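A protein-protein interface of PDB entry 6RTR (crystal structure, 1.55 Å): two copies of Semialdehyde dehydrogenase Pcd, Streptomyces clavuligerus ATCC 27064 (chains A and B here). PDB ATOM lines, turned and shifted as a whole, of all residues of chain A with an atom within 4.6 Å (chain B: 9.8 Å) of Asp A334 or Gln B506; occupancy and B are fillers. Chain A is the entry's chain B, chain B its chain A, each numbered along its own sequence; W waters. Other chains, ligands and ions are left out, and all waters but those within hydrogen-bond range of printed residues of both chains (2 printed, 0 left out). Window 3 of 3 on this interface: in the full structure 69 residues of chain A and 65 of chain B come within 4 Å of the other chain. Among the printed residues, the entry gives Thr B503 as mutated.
O of Asp A334 lies within hydrogen-bond range of NE2 of Gln B506 (3.2 Å).
The side-chain hydroxyl (OG) of Ser A110 sits at hydrogen-bond distance from the side-chain amide oxygen (OE1) of Gln B506.
OG1 of Thr A336 sits close to O of Gln A333 (3.5 Å).
Among the printed residues, pairs that only touch across the chains: Ile A108 with Gln B506 (3.5 Å), Thr A336 with Gln B506 (3.7 Å) and Leu A337 with Ala B505 (3.6 Å).
Asp A334 touches just one residue of chain B: Gln B506.
Printed residues of chain A within 4 Å of Gln B506: Ile A108, Ser A110, Asp A334 and Thr A336.
No residue of chain B comes within 4 Å of Thr A335.
Of the printed residues of chain A, Ala B505 touches Leu A337 (3.6 Å).
Of the printed residues of chain B, Leu A337 touches Ala B505.
Printed residues of chain B within 4 Å of Thr A336: Gln B506.
Of the printed residues of chain B, Ser A110 touches Gln B506.
Printed residues of chain B within 4 Å of Ile A108: Gln B506.
Val B502 touches none of the printed residues of chain A.
The nearest printed residue of chain A that does not touch Ala B505 is Ile A108 (6.3 Å).
Hydrophobic or aromatic side chains of chain B within 4 Å of the printed part of chain A: Ala B505.
Hydrophobic or aromatic side chains of chain A within 4 Å of the printed part of chain B: Ile A108 and Leu A337.
No position is printed for both chains.
Of the 5 pairs that touch across the chains among the printed residues, none has its exchanged pair printed and touching as well.
Water W2 lies within hydrogen-bond range of O of Gln A333 (2.7 Å), O of Thr A336 (2.8 Å) and NE2 of Gln B506 (3.4 Å).
Water W1 lies within hydrogen-bond range of the backbone NH (N) of Ser A110 (3.0 Å) and the side-chain amide nitrogen (NE2) of Gln B506 (3.0 Å).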
ATOM      1  N   ILE A 108      18.175   6.002  -0.119  1.00  0.00           N
ATOM      2  CA  ILE A 108      17.964   4.804   0.705  1.00  0.00           C
ATOM      3  C   ILE A 108      16.796   4.015   0.159  1.00  0.00           C
ATOM      4  O   ILE A 108      15.853   4.560  -0.453  1.00  0.00           O
ATOM      5  CB  ILE A 108      17.851   5.102   2.185  1.00  0.00           C
ATOM      6  CG1 ILE A 108      16.566   5.801   2.576  1.00  0.00           C
ATOM      7  CG2 ILE A 108      19.094   5.829   2.680  1.00  0.00           C
ATOM      8  CD1 ILE A 108      16.466   6.090   4.037  1.00  0.00           C
ATOM      9  N   SER A 110      14.140   2.622   1.357  1.00  0.00           N
ATOM     10  CA  SER A 110      12.793   2.959   1.724  1.00  0.00           C
ATOM     11  C   SER A 110      12.270   4.192   0.932  1.00  0.00           C
ATOM     12  O   SER A 110      11.102   4.256   0.610  1.00  0.00           O
ATOM     13  CB  SER A 110      12.636   3.230   3.193  1.00  0.00           C
ATOM     14  OG  SER A 110      13.437   4.307   3.650  1.00  0.00           O
ATOM     15  N   PHE A 332      21.542   0.559   0.358  1.00  0.00           N
ATOM     16  CA  PHE A 332      20.845  -0.746   0.378  1.00  0.00           C
ATOM     17  C   PHE A 332      20.766  -1.358   1.780  1.00  0.00           C
ATOM     18  O   PHE A 332      20.045  -2.331   1.957  1.00  0.00           O
ATOM     19  CB  PHE A 332      21.532  -1.724  -0.583  1.00  0.00           C
ATOM     20  CG  PHE A 332      21.164  -1.541  -2.012  1.00  0.00           C
ATOM     21  CD1 PHE A 332      19.869  -1.759  -2.427  1.00  0.00           C
ATOM     22  CD2 PHE A 332      22.096  -1.155  -2.936  1.00  0.00           C
ATOM     23  CE1 PHE A 332      19.526  -1.611  -3.746  1.00  0.00           C
ATOM     24  CE2 PHE A 332      21.774  -1.032  -4.277  1.00  0.00           C
ATOM     25  CZ  PHE A 332      20.475  -1.255  -4.675  1.00  0.00           C
ATOM     26  N   GLN A 333      21.410  -0.787   2.780  1.00  0.00           N
ATOM     27  CA  GLN A 333      21.309  -1.280   4.167  1.00  0.00           C
ATOM     28  C   GLN A 333      20.201  -0.551   4.874  1.00  0.00           C
ATOM     29  O   GLN A 333      20.167   0.677   4.907  1.00  0.00           O
ATOM     30  CB  GLN A 333      22.636  -1.089   4.925  1.00  0.00           C
ATOM     31  CG  GLN A 333      23.785  -1.909   4.370  1.00  0.00           C
ATOM     32  CD  GLN A 333      23.602  -3.412   4.567  1.00  0.00           C
ATOM     33  OE1 GLN A 333      22.791  -3.842   5.373  1.00  0.00           O
ATOM     34  NE2 GLN A 333      24.359  -4.210   3.825  1.00  0.00           N
ATOM     35  N   ASP A 334      19.269  -1.290   5.474  1.00  0.00           N
ATOM     36  CA  ASP A 334      18.158  -0.670   6.143  1.00  0.00           C
ATOM     37  C   ASP A 334      18.499   0.172   7.361  1.00  0.00           C
ATOM     38  O   ASP A 334      17.733   1.025   7.753  1.00  0.00           O
ATOM     39  CB  ASP A 334      17.156  -1.749   6.595  1.00  0.00           C
ATOM     40  CG  ASP A 334      16.364  -2.364   5.428  1.00  0.00           C
ATOM     41  OD1 ASP A 334      16.166  -1.698   4.384  1.00  0.00           O
ATOM     42  OD2 ASP A 334      15.908  -3.508   5.605  1.00  0.00           O
ATOM     43  N   THR A 335      19.653  -0.058   7.953  1.00  0.00           N
ATOM     44  CA  THR A 335      20.144   0.770   9.033  1.00  0.00           C
ATOM     45  C   THR A 335      20.516   2.204   8.604  1.00  0.00           C
ATOM     46  O   THR A 335      20.580   3.101   9.430  1.00  0.00           O
ATOM     47  CB  THR A 335      21.378   0.136   9.707  1.00  0.00           C
ATOM     48  OG1 THR A 335      22.325  -0.284   8.721  1.00  0.00           O
ATOM     49  CG2 THR A 335      20.912  -1.086  10.507  1.00  0.00           C
ATOM     50  N   THR A 336      20.756   2.389   7.339  1.00  0.00           N
ATOM     51  CA  THR A 336      21.219   3.722   6.863  1.00  0.00           C
ATOM     52  C   THR A 336      20.075   4.750   6.822  1.00  0.00           C
ATOM     53  O   THR A 336      19.011   4.431   6.364  1.00  0.00           O
ATOM     54  CB  THR A 336      21.760   3.564   5.456  1.00  0.00           C
ATOM     55  OG1 THR A 336      22.915   2.706   5.481  1.00  0.00           O
ATOM     56  CG2 THR A 336      22.117   4.950   4.809  1.00  0.00           C
ATOM     57  N   LEU A 337      20.316   5.962   7.295  1.00  0.00           N
ATOM     58  CA  LEU A 337      19.419   7.097   7.129  1.00  0.00           C
ATOM     59  C   LEU A 337      19.947   8.012   6.021  1.00  0.00           C
ATOM     60  O   LEU A 337      19.157   8.567   5.291  1.00  0.00           O
ATOM     61  CB  LEU A 337      19.207   7.878   8.413  1.00  0.00           C
ATOM     62  CG  LEU A 337      18.303   9.129   8.298  1.00  0.00           C
ATOM     63  CD1 LEU A 337      16.948   8.820   7.647  1.00  0.00           C
ATOM     64  CD2 LEU A 337      18.075   9.773   9.661  1.00  0.00           C
ATOM     65  N   VAL B 502       5.153  13.019  13.969  1.00  0.00           N
ATOM     66  CA  VAL B 502       5.688  12.977  12.642  1.00  0.00           C
ATOM     67  C   VAL B 502       6.162  11.579  12.307  1.00  0.00           C
ATOM     68  O   VAL B 502       6.612  10.866  13.195  1.00  0.00           O
ATOM     69  CB  VAL B 502       6.890  13.967  12.474  1.00  0.00           C
ATOM     70  CG1 VAL B 502       8.036  13.693  13.435  1.00  0.00           C
ATOM     71  CG2 VAL B 502       7.421  13.977  11.032  1.00  0.00           C
ATOM     72  N   THR B 503       6.122  11.211  11.039  1.00  0.00           N
ATOM     73  CA  THR B 503       6.762   9.977  10.575  1.00  0.00           C
ATOM     74  C   THR B 503       8.216   9.943  10.921  1.00  0.00           C
ATOM     75  O   THR B 503       8.960  10.902  10.681  1.00  0.00           O
ATOM     76  CB  THR B 503       6.620   9.836   9.058  1.00  0.00           C
ATOM     77  OG1 THR B 503       5.230   9.875   8.747  1.00  0.00           O
ATOM     78  CG2 THR B 503       7.263   8.537   8.546  1.00  0.00           C
ATOM     79  N   LEU B 504       8.635   8.852  11.555  1.00  0.00           N
ATOM     80  CA  LEU B 504      10.015   8.729  11.969  1.00  0.00           C
ATOM     81  C   LEU B 504      10.780   7.980  10.912  1.00  0.00           C
ATOM     82  O   LEU B 504      10.418   6.864  10.538  1.00  0.00           O
ATOM     83  CB  LEU B 504      10.112   7.981  13.283  1.00  0.00           C
ATOM     84  CG  LEU B 504       9.332   8.627  14.414  1.00  0.00           C
ATOM     85  CD1 LEU B 504       9.346   7.697  15.607  1.00  0.00           C
ATOM     86  CD2 LEU B 504       9.876   9.969  14.820  1.00  0.00           C
ATOM     87  N   ALA B 505      11.829   8.586  10.407  1.00  0.00           N
ATOM     88  CA  ALA B 505      12.555   8.018   9.290  1.00  0.00           C
ATOM     89  C   ALA B 505      13.316   6.760   9.749  1.00  0.00           C
ATOM     90  O   ALA B 505      14.098   6.803  10.725  1.00  0.00           O
ATOM     91  CB  ALA B 505      13.537   9.027   8.737  1.00  0.00           C
ATOM     92  N   GLN B 506      13.063   5.674   9.038  1.00  0.00           N
ATOM     93  CA  GLN B 506      13.570   4.346   9.401  1.00  0.00           C
ATOM     94  C   GLN B 506      13.182   3.937  10.807  1.00  0.00           C
ATOM     95  O   GLN B 506      13.848   3.078  11.401  1.00  0.00           O
ATOM     96  CB  GLN B 506      15.115   4.307   9.234  1.00  0.00           C
ATOM     97  CG  GLN B 506      15.605   4.865   7.911  1.00  0.00           C
ATOM     98  CD  GLN B 506      15.031   4.121   6.744  1.00  0.00           C
ATOM     99  OE1 GLN B 506      14.063   4.570   6.098  1.00  0.00           O
ATOM    100  NE2 GLN B 506      15.607   2.994   6.463  1.00  0.00           N
ATOM    101  N   GLY B 507      12.102   4.538  11.330  1.00  0.00           N
ATOM    102  CA  GLY B 507      11.650   4.322  12.703  1.00  0.00           C
ATOM    103  C   GLY B 507      12.450   4.938  13.824  1.00  0.00           C
ATOM    104  O   GLY B 507      12.184   4.663  14.984  1.00  0.00           O
ATOM    105  N   VAL B 508      13.459   5.767  13.520  1.00  0.00           N
ATOM    106  CA  VAL B 508      14.329   6.300  14.548  1.00  0.00           C
ATOM    107  C   VAL B 508      13.714   7.504  15.243  1.00  0.00           C
ATOM    108  O   VAL B 508      13.282   8.446  14.571  1.00  0.00           O
ATOM    109  CB  VAL B 508      15.684   6.704  13.944  1.00  0.00           C
ATOM    110  CG1 VAL B 508      16.581   7.287  15.018  1.00  0.00           C
ATOM    111  CG2 VAL B 508      16.346   5.506  13.291  1.00  0.00           C
ATOM    112  N   ASP B 509      13.704   7.515  16.577  1.00  0.00           N
ATOM    113  CA  ASP B 509      13.208   8.694  17.317  1.00  0.00           C
ATOM    114  C   ASP B 509      14.394   9.477  17.909  1.00  0.00           C
ATOM    115  O   ASP B 509      15.016   9.012  18.859  1.00  0.00           O
ATOM    116  CB  ASP B 509      12.223   8.247  18.404  1.00  0.00           C
ATOM    117  CG  ASP B 509      11.550   9.410  19.100  1.00  0.00           C
ATOM    118  OD1 ASP B 509      12.002  10.548  18.892  1.00  0.00           O
ATOM    119  OD2 ASP B 509      10.574   9.189  19.861  1.00  0.00           O
ATOM    120  N   PHE B 510      14.741  10.633  17.346  1.00  0.00           N
ATOM    121  CA  PHE B 510      15.923  11.418  17.815  1.00  0.00           C
ATOM    122  C   PHE B 510      15.746  11.948  19.257  1.00  0.00           C
ATOM    123  O   PHE B 510      16.564  12.669  19.842  1.00  0.00           O
ATOM    124  CB  PHE B 510      16.270  12.432  16.743  1.00  0.00           C
ATOM    125  CG  PHE B 510      17.056  11.674  15.735  1.00  0.00           C
ATOM    126  CD1 PHE B 510      18.333  11.272  16.046  1.00  0.00           C
ATOM    127  CD2 PHE B 510      16.516  11.340  14.510  1.00  0.00           C
ATOM    128  CE1 PHE B 510      19.076  10.585  15.131  1.00  0.00           C
ATOM    129  CE2 PHE B 510      17.256  10.663  13.570  1.00  0.00           C
ATOM    130  CZ  PHE B 510      18.553  10.285  13.894  1.00  0.00           C
HETATM  131  O   HOH W   1      15.719   1.790   3.727  1.00  0.00           O
HETATM  132  O   HOH W   2      18.257   2.564   4.358  1.00  0.00           O
